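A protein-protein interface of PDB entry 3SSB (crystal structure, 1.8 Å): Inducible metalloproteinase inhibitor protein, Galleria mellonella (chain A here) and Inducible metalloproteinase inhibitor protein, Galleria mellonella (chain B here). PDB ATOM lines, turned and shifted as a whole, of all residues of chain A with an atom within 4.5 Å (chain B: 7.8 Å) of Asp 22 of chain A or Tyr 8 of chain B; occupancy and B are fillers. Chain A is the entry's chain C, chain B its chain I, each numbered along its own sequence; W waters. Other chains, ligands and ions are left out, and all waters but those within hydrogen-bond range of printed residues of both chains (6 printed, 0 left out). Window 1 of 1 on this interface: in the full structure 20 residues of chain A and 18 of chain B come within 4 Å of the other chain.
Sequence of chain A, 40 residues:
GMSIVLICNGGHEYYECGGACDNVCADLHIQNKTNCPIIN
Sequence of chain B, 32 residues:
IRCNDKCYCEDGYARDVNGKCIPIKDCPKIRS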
ATOM      1  N   HIS A  12      12.336  37.787  20.452  1.00  0.00           N
ATOM      2  CA  HIS A  12      11.279  37.177  19.671  1.00  0.00           C
ATOM      3  C   HIS A  12      10.669  35.905  20.316  1.00  0.00           C
ATOM      4  O   HIS A  12      10.208  34.990  19.615  1.00  0.00           O
ATOM      5  CB  HIS A  12      11.768  36.904  18.243  1.00  0.00           C
ATOM      6  CG  HIS A  12      11.904  38.143  17.415  1.00  0.00           C
ATOM      7  ND1 HIS A  12      13.122  38.612  16.976  1.00  0.00           N
ATOM      8  CD2 HIS A  12      10.975  39.016  16.963  1.00  0.00           C
ATOM      9  CE1 HIS A  12      12.938  39.717  16.276  1.00  0.00           C
ATOM     10  NE2 HIS A  12      11.644  39.983  16.250  1.00  0.00           N
ATOM     11  N   GLU A  13      10.628  35.865  21.648  1.00  0.00           N
ATOM     12  CA  GLU A  13       9.969  34.752  22.326  1.00  0.00           C
ATOM     13  C   GLU A  13       9.110  35.274  23.466  1.00  0.00           C
ATOM     14  O   GLU A  13       9.200  36.450  23.843  1.00  0.00           O
ATOM     15  CB  GLU A  13      11.013  33.742  22.827  1.00  0.00           C
ATOM     16  CG  GLU A  13      12.077  34.355  23.708  1.00  0.00           C
ATOM     17  CD  GLU A  13      12.959  33.356  24.471  1.00  0.00           C
ATOM     18  OE1 GLU A  13      12.818  32.120  24.341  1.00  0.00           O
ATOM     19  OE2 GLU A  13      13.823  33.840  25.223  1.00  0.00           O
ATOM     20  N   TYR A  14       8.297  34.388  24.028  1.00  0.00           N
ATOM     21  CA  TYR A  14       7.392  34.741  25.113  1.00  0.00           C
ATOM     22  C   TYR A  14       7.028  33.515  25.919  1.00  0.00           C
ATOM     23  O   TYR A  14       7.086  32.387  25.417  1.00  0.00           O
ATOM     24  CB  TYR A  14       6.107  35.404  24.567  1.00  0.00           C
ATOM     25  CG  TYR A  14       5.297  34.471  23.707  1.00  0.00           C
ATOM     26  CD1 TYR A  14       4.345  33.631  24.260  1.00  0.00           C
ATOM     27  CD2 TYR A  14       5.538  34.379  22.340  1.00  0.00           C
ATOM     28  CE1 TYR A  14       3.626  32.732  23.459  1.00  0.00           C
ATOM     29  CE2 TYR A  14       4.844  33.515  21.556  1.00  0.00           C
ATOM     30  CZ  TYR A  14       3.885  32.692  22.104  1.00  0.00           C
ATOM     31  OH  TYR A  14       3.201  31.813  21.283  1.00  0.00           O
ATOM     32  N   GLU A  16       4.332  31.136  27.905  1.00  0.00           N
ATOM     33  CA  GLU A  16       2.956  30.686  28.030  1.00  0.00           C
ATOM     34  C   GLU A  16       2.988  29.282  28.608  1.00  0.00           C
ATOM     35  O   GLU A  16       3.980  28.574  28.458  1.00  0.00           O
ATOM     36  CB  GLU A  16       2.252  30.659  26.676  1.00  0.00           C
ATOM     37  CG  GLU A  16       0.798  30.204  26.753  1.00  0.00           C
ATOM     38  CD  GLU A  16       0.165  29.996  25.388  1.00  0.00           C
ATOM     39  OE1 GLU A  16      -0.450  28.932  25.161  1.00  0.00           O
ATOM     40  OE2 GLU A  16       0.262  30.925  24.551  1.00  0.00           O
ATOM     41  N   CYS A  17       1.930  28.907  29.314  1.00  0.00           N
ATOM     42  CA  CYS A  17       1.700  27.522  29.628  1.00  0.00           C
ATOM     43  C   CYS A  17       0.803  27.013  28.518  1.00  0.00           C
ATOM     44  O   CYS A  17      -0.416  27.199  28.572  1.00  0.00           O
ATOM     45  CB  CYS A  17       1.047  27.322  30.990  1.00  0.00           C
ATOM     46  SG  CYS A  17       1.265  25.612  31.598  1.00  0.00           S
ATOM     47  N   GLY A  18       1.430  26.400  27.518  1.00  0.00           N
ATOM     48  CA  GLY A  18       0.763  26.087  26.265  1.00  0.00           C
ATOM     49  C   GLY A  18       1.015  24.674  25.791  1.00  0.00           C
ATOM     50  O   GLY A  18       1.285  23.777  26.575  1.00  0.00           O
ATOM     51  N   GLY A  19       0.920  24.494  24.471  1.00  0.00           N
ATOM     52  CA  GLY A  19       1.187  23.233  23.836  1.00  0.00           C
ATOM     53  C   GLY A  19       2.629  22.790  23.821  1.00  0.00           C
ATOM     54  O   GLY A  19       3.556  23.536  24.118  1.00  0.00           O
ATOM     55  N   ALA A  20       2.830  21.537  23.463  1.00  0.00           N
ATOM     56  CA  ALA A  20       4.145  20.942  23.566  1.00  0.00           C
ATOM     57  C   ALA A  20       5.135  21.402  22.472  1.00  0.00           C
ATOM     58  O   ALA A  20       6.357  21.289  22.656  1.00  0.00           O
ATOM     59  CB  ALA A  20       4.027  19.401  23.561  1.00  0.00           C
ATOM     60  N   CYS A  21       4.623  21.874  21.332  1.00  0.00           N
ATOM     61  CA  CYS A  21       5.495  22.191  20.202  1.00  0.00           C
ATOM     62  C   CYS A  21       5.821  23.678  20.176  1.00  0.00           C
ATOM     63  O   CYS A  21       4.958  24.504  20.359  1.00  0.00           O
ATOM     64  CB  CYS A  21       4.851  21.792  18.873  1.00  0.00           C
ATOM     65  SG  CYS A  21       4.462  20.026  18.735  1.00  0.00           S
ATOM     66  N   ASP A  22       7.082  23.980  19.953  1.00  0.00           N
ATOM     67  CA  ASP A  22       7.526  25.321  19.554  1.00  0.00           C
ATOM     68  C   ASP A  22       7.726  25.311  18.028  1.00  0.00           C
ATOM     69  O   ASP A  22       7.614  24.262  17.377  1.00  0.00           O
ATOM     70  CB  ASP A  22       8.853  25.634  20.242  1.00  0.00           C
ATOM     71  CG  ASP A  22       9.217  27.135  20.267  1.00  0.00           C
ATOM     72  OD1 ASP A  22       8.517  27.993  19.664  1.00  0.00           O
ATOM     73  OD2 ASP A  22      10.269  27.424  20.914  1.00  0.00           O
ATOM     74  N   ASN A  23       8.032  26.478  17.471  1.00  0.00           N
ATOM     75  CA  ASN A  23       8.545  26.581  16.112  1.00  0.00           C
ATOM     76  C   ASN A  23      10.038  26.377  16.152  1.00  0.00           C
ATOM     77  O   ASN A  23      10.745  27.189  16.741  1.00  0.00           O
ATOM     78  CB  ASN A  23       8.279  27.966  15.523  1.00  0.00           C
ATOM     79  CG  ASN A  23       6.826  28.205  15.201  1.00  0.00           C
ATOM     80  OD1 ASN A  23       6.010  27.291  15.216  1.00  0.00           O
ATOM     81  ND2 ASN A  23       6.490  29.463  14.905  1.00  0.00           N
ATOM     82  N   VAL A  24      10.519  25.290  15.547  1.00  0.00           N
ATOM     83  CA  VAL A  24      11.952  24.991  15.506  1.00  0.00           C
ATOM     84  C   VAL A  24      12.331  24.792  14.035  1.00  0.00           C
ATOM     85  O   VAL A  24      11.688  23.997  13.340  1.00  0.00           O
ATOM     86  CB  VAL A  24      12.286  23.724  16.331  1.00  0.00           C
ATOM     87  CG1 VAL A  24      13.755  23.388  16.232  1.00  0.00           C
ATOM     88  CG2 VAL A  24      11.878  23.888  17.807  1.00  0.00           C
ATOM     89  N   ASN A  32       4.784  22.388  14.261  1.00  0.00           N
ATOM     90  CA  ASN A  32       4.999  23.767  14.694  1.00  0.00           C
ATOM     91  C   ASN A  32       4.014  24.062  15.809  1.00  0.00           C
ATOM     92  O   ASN A  32       3.313  23.162  16.256  1.00  0.00           O
ATOM     93  CB  ASN A  32       4.847  24.735  13.505  1.00  0.00           C
ATOM     94  CG  ASN A  32       3.512  24.608  12.813  1.00  0.00           C
ATOM     95  OD1 ASN A  32       2.466  24.849  13.411  1.00  0.00           O
ATOM     96  ND2 ASN A  32       3.538  24.249  11.518  1.00  0.00           N
ATOM     97  N   LYS A  33       3.957  25.305  16.272  1.00  0.00           N
ATOM     98  CA  LYS A  33       3.074  25.657  17.388  1.00  0.00           C
ATOM     99  C   LYS A  33       1.618  25.273  17.189  1.00  0.00           C
ATOM    100  O   LYS A  33       0.963  24.839  18.151  1.00  0.00           O
ATOM    101  CB  LYS A  33       3.123  27.160  17.669  1.00  0.00           C
ATOM    102  CG  LYS A  33       4.422  27.615  18.275  1.00  0.00           C
ATOM    103  CD  LYS A  33       4.319  29.030  18.898  1.00  0.00           C
ATOM    104  CE  LYS A  33       4.068  30.099  17.925  1.00  0.00           C
ATOM    105  NZ  LYS A  33       3.845  31.464  18.593  1.00  0.00           N
ATOM    106  N   CYS B   3      -0.671  21.709  30.552  1.00  0.00           N
ATOM    107  CA  CYS B   3       0.049  22.618  29.655  1.00  0.00           C
ATOM    108  C   CYS B   3       1.538  22.569  29.976  1.00  0.00           C
ATOM    109  O   CYS B   3       1.938  22.028  31.009  1.00  0.00           O
ATOM    110  CB  CYS B   3      -0.521  24.033  29.703  1.00  0.00           C
ATOM    111  SG  CYS B   3      -0.581  24.797  31.303  1.00  0.00           S
ATOM    112  N   ASN B   4       2.346  23.178  29.098  1.00  0.00           N
ATOM    113  CA  ASN B   4       3.792  23.206  29.192  1.00  0.00           C
ATOM    114  C   ASN B   4       4.282  24.603  29.499  1.00  0.00           C
ATOM    115  O   ASN B   4       4.013  25.550  28.746  1.00  0.00           O
ATOM    116  CB  ASN B   4       4.410  22.792  27.853  1.00  0.00           C
ATOM    117  CG  ASN B   4       4.025  21.372  27.449  1.00  0.00           C
ATOM    118  OD1 ASN B   4       4.700  20.424  27.836  1.00  0.00           O
ATOM    119  ND2 ASN B   4       2.931  21.236  26.730  1.00  0.00           N
ATOM    120  N   ASP B   5       5.009  24.742  30.595  1.00  0.00           N
ATOM    121  CA  ASP B   5       5.578  26.043  30.933  1.00  0.00           C
ATOM    122  C   ASP B   5       6.834  26.234  30.100  1.00  0.00           C
ATOM    123  O   ASP B   5       7.873  25.641  30.404  1.00  0.00           O
ATOM    124  CB  ASP B   5       5.885  26.118  32.400  1.00  0.00           C
ATOM    125  CG  ASP B   5       4.635  26.073  33.235  1.00  0.00           C
ATOM    126  OD1 ASP B   5       3.765  26.953  33.049  1.00  0.00           O
ATOM    127  OD2 ASP B   5       4.521  25.147  34.054  1.00  0.00           O
ATOM    128  N   LYS B   6       6.719  27.050  29.050  1.00  0.00           N
ATOM    129  CA  LYS B   6       7.710  27.108  27.983  1.00  0.00           C
ATOM    130  C   LYS B   6       7.923  28.520  27.496  1.00  0.00           C
ATOM    131  O   LYS B   6       6.995  29.323  27.546  1.00  0.00           O
ATOM    132  CB  LYS B   6       7.185  26.347  26.754  1.00  0.00           C
ATOM    133  CG  LYS B   6       7.680  24.959  26.655  1.00  0.00           C
ATOM    134  CD  LYS B   6       7.114  24.276  25.441  1.00  0.00           C
ATOM    135  CE  LYS B   6       7.975  24.476  24.212  1.00  0.00           C
ATOM    136  NZ  LYS B   6       9.120  23.607  24.306  1.00  0.00           N
ATOM    137  N   CYS B   7       9.099  28.784  26.942  1.00  0.00           N
ATOM    138  CA  CYS B   7       9.262  29.936  26.054  1.00  0.00           C
ATOM    139  C   CYS B   7       8.926  29.488  24.641  1.00  0.00           C
ATOM    140  O   CYS B   7       9.375  28.429  24.216  1.00  0.00           O
ATOM    141  CB  CYS B   7      10.680  30.502  26.089  1.00  0.00           C
ATOM    142  SG  CYS B   7      11.149  31.113  27.707  1.00  0.00           S
ATOM    143  N   TYR B   8       8.138  30.287  23.924  1.00  0.00           N
ATOM    144  CA  TYR B   8       7.815  30.008  22.526  1.00  0.00           C
ATOM    145  C   TYR B   8       8.305  31.131  21.632  1.00  0.00           C
ATOM    146  O   TYR B   8       8.285  32.289  22.032  1.00  0.00           O
ATOM    147  CB  TYR B   8       6.291  29.893  22.322  1.00  0.00           C
ATOM    148  CG  TYR B   8       5.625  28.827  23.143  1.00  0.00           C
ATOM    149  CD1 TYR B   8       5.398  27.568  22.615  1.00  0.00           C
ATOM    150  CD2 TYR B   8       5.248  29.066  24.467  1.00  0.00           C
ATOM    151  CE1 TYR B   8       4.784  26.575  23.377  1.00  0.00           C
ATOM    152  CE2 TYR B   8       4.631  28.084  25.215  1.00  0.00           C
ATOM    153  CZ  TYR B   8       4.390  26.840  24.649  1.00  0.00           C
ATOM    154  OH  TYR B   8       3.778  25.849  25.382  1.00  0.00           O
ATOM    155  N   CYS B   9       8.751  30.795  20.418  1.00  0.00           N
ATOM    156  CA  CYS B   9       8.997  31.822  19.429  1.00  0.00           C
ATOM    157  C   CYS B   9       7.681  32.424  19.009  1.00  0.00           C
ATOM    158  O   CYS B   9       6.667  31.726  18.937  1.00  0.00           O
ATOM    159  CB  CYS B   9       9.666  31.253  18.186  1.00  0.00           C
ATOM    160  SG  CYS B   9      11.320  30.616  18.450  1.00  0.00           S
ATOM    161  N   GLU B  10       7.708  33.728  18.748  1.00  0.00           N
ATOM    162  CA  GLU B  10       6.601  34.427  18.128  1.00  0.00           C
ATOM    163  C   GLU B  10       6.265  33.807  16.781  1.00  0.00           C
ATOM    164  O   GLU B  10       7.120  33.173  16.130  1.00  0.00           O
ATOM    165  CB  GLU B  10       6.950  35.911  17.922  1.00  0.00           C
ATOM    166  CG  GLU B  10       7.171  36.721  19.231  1.00  0.00           C
ATOM    167  CD  GLU B  10       7.483  38.180  18.974  1.00  0.00           C
ATOM    168  OE1 GLU B  10       8.120  38.846  19.841  1.00  0.00           O
ATOM    169  OE2 GLU B  10       7.114  38.687  17.897  1.00  0.00           O
ATOM    170  N   ASP B  11       5.010  33.980  16.368  1.00  0.00           N
ATOM    171  CA  ASP B  11       4.606  33.570  15.023  1.00  0.00           C
ATOM    172  C   ASP B  11       5.519  34.308  14.030  1.00  0.00           C
ATOM    173  O   ASP B  11       5.759  35.528  14.158  1.00  0.00           O
ATOM    174  CB  ASP B  11       3.157  33.886  14.734  1.00  0.00           C
ATOM    175  CG  ASP B  11       2.185  33.138  15.625  1.00  0.00           C
ATOM    176  OD1 ASP B  11       2.517  32.086  16.199  1.00  0.00           O
ATOM    177  OD2 ASP B  11       1.040  33.602  15.711  1.00  0.00           O
ATOM    178  N   TYR B  13       8.631  33.194  13.565  1.00  0.00           N
ATOM    179  CA  TYR B  13       9.959  32.976  14.096  1.00  0.00           C
ATOM    180  C   TYR B  13      10.092  31.531  14.555  1.00  0.00           C
ATOM    181  O   TYR B  13       9.097  30.853  14.822  1.00  0.00           O
ATOM    182  CB  TYR B  13      10.219  33.986  15.218  1.00  0.00           C
ATOM    183  CG  TYR B  13      10.301  35.406  14.687  1.00  0.00           C
ATOM    184  CD1 TYR B  13       9.154  36.131  14.380  1.00  0.00           C
ATOM    185  CD2 TYR B  13      11.528  36.020  14.487  1.00  0.00           C
ATOM    186  CE1 TYR B  13       9.228  37.428  13.874  1.00  0.00           C
ATOM    187  CE2 TYR B  13      11.612  37.314  13.965  1.00  0.00           C
ATOM    188  CZ  TYR B  13      10.453  38.007  13.659  1.00  0.00           C
ATOM    189  OH  TYR B  13      10.539  39.288  13.169  1.00  0.00           O
ATOM    190  N   ALA B  14      11.328  31.051  14.567  1.00  0.00           N
ATOM    191  CA  ALA B  14      11.631  29.669  14.888  1.00  0.00           C
ATOM    192  C   ALA B  14      13.046  29.578  15.452  1.00  0.00           C
ATOM    193  O   ALA B  14      13.904  30.406  15.144  1.00  0.00           O
ATOM    194  CB  ALA B  14      11.504  28.796  13.668  1.00  0.00           C
ATOM    195  N   ARG B  15      13.254  28.547  16.261  1.00  0.00           N
ATOM    196  CA  ARG B  15      14.528  28.312  16.959  1.00  0.00           C
ATOM    197  C   ARG B  15      15.618  27.883  15.977  1.00  0.00           C
ATOM    198  O   ARG B  15      15.420  26.936  15.210  1.00  0.00           O
ATOM    199  CB  ARG B  15      14.356  27.209  18.004  1.00  0.00           C
ATOM    200  CG  ARG B  15      13.326  27.491  19.085  1.00  0.00           C
ATOM    201  CD  ARG B  15      13.823  28.491  20.125  1.00  0.00           C
ATOM    202  NE  ARG B  15      12.745  28.848  21.039  1.00  0.00           N
ATOM    203  CZ  ARG B  15      12.832  29.749  22.012  1.00  0.00           C
ATOM    204  NH1 ARG B  15      13.963  30.421  22.238  1.00  0.00           N
ATOM    205  NH2 ARG B  15      11.770  29.983  22.767  1.00  0.00           N
ATOM    206  N   GLY B  19      19.450  28.007  19.609  1.00  0.00           N
ATOM    207  CA  GLY B  19      18.248  28.110  20.451  1.00  0.00           C
ATOM    208  C   GLY B  19      17.598  29.485  20.457  1.00  0.00           C
ATOM    209  O   GLY B  19      16.717  29.764  21.284  1.00  0.00           O
ATOM    210  N   CYS B  21      15.359  32.448  18.707  1.00  0.00           N
ATOM    211  CA  CYS B  21      14.274  32.638  17.752  1.00  0.00           C
ATOM    212  C   CYS B  21      14.726  33.627  16.689  1.00  0.00           C
ATOM    213  O   CYS B  21      15.065  34.771  17.004  1.00  0.00           O
ATOM    214  CB  CYS B  21      13.003  33.144  18.446  1.00  0.00           C
ATOM    215  SG  CYS B  21      12.288  31.994  19.615  1.00  0.00           S
HETATM  216  O   HOH W   1       8.470  38.534  22.375  1.00  0.00           O
HETATM  217  O   HOH W   2       1.770  27.089  34.777  1.00  0.00           O
HETATM  218  O   HOH W   3      14.124  30.311  25.826  1.00  0.00           O
HETATM  219  O   HOH W   4       8.789  40.922  15.714  1.00  0.00           O
HETATM  220  O   HOH W   5      16.215  32.585  23.602  1.00  0.00           O
HETATM  221  O   HOH W   6       3.611  30.050  14.387  1.00  0.00           O
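Water W1 bridges the side-chain carboxylate of Glu 10 of chain B (2.6 Å) and the backbone carbonyl oxygen of Glu 13 of chain A (2.7 Å). Water W2 lies within hydrogen-bond range of the side-chain carboxylate of Asp 5 of chain B and the side-chain sulfur of Cys 17 of chain A. Water W3 bridges the side-chain carboxylate (OE1) of Glu 13 of chain A (2.7 Å) and the side-chain sulfur (SG) of Cys 7 of chain B (3.6 Å). Water W6 bridges the side-chain carboxylate of Asp 11 of chain B (2.9 Å) and the side-chain amide nitrogen of Asn 23 of chain A (3.0 Å). Water W4 lies within hydrogen-bond range of NE2 of His 12 of chain A and OH of Tyr 13 of chain B. Water W5 lies within hydrogen-bond range of the side-chain carboxylate of Glu 13 of chain A (3.2 Å) and the guanidinium group of Arg 15 of chain B (3.4 Å).
His 12 of chain A touches Cys 9 of chain B (O to CA, 3.4 Å). OE1 of Glu 13 of chain A touches CB of Cys 7 of chain B, 3.2 Å away. Glu 13 of chain A touches Tyr 8 of chain B (CA to O, 3.0 Å). O of Lys 6 of chain B touches O of Tyr 14 of chain A, 3.7 Å away. Cys 9 of chain B touches Tyr 14 of chain A. Glu 10 of chain B touches Tyr 14 of chain A. ND2 of Asn 4 of chain B touches C of Gly 19 of chain A, at 3.3 Å. O of Gly 19 of chain A touches CD of Lys 6 of chain B (3.9 Å). CA of Ala 14 of chain B touches O of Asn 23 of chain A, 3.2 Å away. N of Arg 15 of chain B touches CA of Val 24 of chain A, 3.9 Å away.
The side-chain hydroxyl (OH) of Tyr 14 of chain A lies within hydrogen-bond range of the side-chain amino group (NZ) of Lys 33 of chain A (2.8 Å). The side-chain amide oxygen (OD1) of Asn 23 of chain A is in hydrogen-bond range of the backbone NH (N) of Lys 33 of chain A (3.0 Å). The backbone carbonyl oxygen (O) of Asn 4 of chain B lies within hydrogen-bond range of the side-chain hydroxyl (OH) of Tyr 8 of chain B (3.4 Å). O of Cys 7 of chain B lies within hydrogen-bond range of NH2 of Arg 15 of chain B. The guanidinium group (NH1) of Arg 15 of chain B lies within hydrogen-bond range of the backbone carbonyl oxygen (O) of Gly 19 of chain B. The guanidinium group (NE) of Arg 15 of chain B sits close to the side-chain sulfur (SG) of Cys 21 of chain B, 3.5 Å away.
Of chain B, only Cys 7, Tyr 8, Cys 9 and Arg 15 come within 4 Å of Asp 22 of chain A. Tyr 8 of chain B touches seven residues of chain A. Of the printed residues of chain A, Cys 7 of chain B touches Glu 13 (3.2 Å), Tyr 14 (3.3 Å) and Asp 22 (3.6 Å). Of the printed residues of chain B, Glu 13 of chain A touches Cys 7 (3.2 Å), Tyr 8 (3.0 Å), Arg 15 (2.9 Å) and Cys 21 (3.9 Å). Of the printed residues of chain B, Cys 21 of chain A touches Tyr 8. Of the printed residues of chain A, Asp 5 of chain B touches Glu 16 (3.9 Å) and Cys 17 (3.2 Å). Printed residues of chain A within 4 Å of Lys 6 of chain B: Tyr 14, Glu 16, Gly 19 and Ala 20. Gly 19 of chain B touches none of the printed residues of chain A. Asn 32 of chain A touches none of the printed residues of chain B.
Of the 14 printed residues of chain A, 13 touch a printed residue of chain B. Hydrophobic or aromatic side chains of chain A that line the printed part of chain B: His 12, Tyr 14 and Ala 20. Of the 14 printed residues of chain B, 13 touch a printed residue of chain A. Along chain B the printed residues that touch a printed residue of chain A span positions 3 to 21. Among the printed residues, Asp or Glu carboxylates within 4 Å of a Lys or Arg side-chain nitrogen of the other chain: Glu 13 of chain A with Arg 15 of chain B (2.9 Å), Asp 22 of chain A with Arg 15 of chain B (2.9 Å) and Lys 33 of chain A with Asp 11 of chain B (2.8 Å).
The backbone carbonyl oxygen (O) of His 12 of chain A sits at hydrogen-bond distance from the backbone NH (N) of Glu 10 of chain B (2.9 Å). A ring nitrogen (NE2) of His 12 of chain A sits at hydrogen-bond distance from the side-chain hydroxyl of Tyr 13 of chain B, at 3.3 Å. The side-chain carboxylate (OE1) of Glu 13 of chain A is in salt-bridge range of the guanidinium group (NH2) of Arg 15 of chain B, 2.9 Å away. N of Tyr 8 of chain B lies within hydrogen-bond range of O of Tyr 14 of chain A (2.8 Å). The backbone carbonyl oxygen (O) of Glu 16 of chain A is in hydrogen-bond range of the backbone NH (N) of Lys 6 of chain B, 3.2 Å away. The side-chain sulfur of Cys 17 of chain A forms a disulfide with the side-chain sulfur of Cys 3 of chain B. SG of Cys 17 of chain A lies within hydrogen-bond range of N of Asn 4 of chain B. The backbone carbonyl oxygen of Gly 18 of chain A lies within hydrogen-bond range of the backbone NH of Asn 4 of chain B (2.8 Å). The backbone NH (N) of Gly 18 of chain A sits close to the side-chain hydroxyl (OH) of Tyr 8 of chain B (3.2 Å). The side-chain hydroxyl of Tyr 8 of chain B sits at hydrogen-bond distance from the backbone carbonyl oxygen of Gly 19 of chain A (2.6 Å). The side-chain amide nitrogen (ND2) of Asn 4 of chain B sits close to the backbone NH (N) of Ala 20 of chain A, 3.3 Å away. The backbone NH of Cys 9 of chain B lies within hydrogen-bond range of the side-chain carboxylate of Asp 22 of chain A (2.9 Å). The side-chain carboxylate (OD2) of Asp 22 of chain A is in salt-bridge range of the guanidinium group (NE) of Arg 15 of chain B, at 2.9 Å. The backbone carbonyl oxygen (O) of Tyr 13 of chain B lies within hydrogen-bond range of the side-chain amide nitrogen (ND2) of Asn 23 of chain A, 3.0 Å away. O of Asn 23 of chain A sits at hydrogen-bond distance from N of Arg 15 of chain B, at 2.9 Å. NZ of Lys 33 of chain A sits at hydrogen-bond distance from O of Cys 9 of chain B (2.9 Å). NZ of Lys 33 of chain A is in salt-bridge range of OD1 of Asp 11 of chain B (2.8 Å). SG of Cys 21 of chain B lies close to O of His 12 of chain A. O of Asn 4 of chain B sits close to O of Glu 16 of chain A, at 3.0 Å. SG of Cys 17 of chain A lies close to OD1 of Asp 5 of chain B (3.2 Å).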
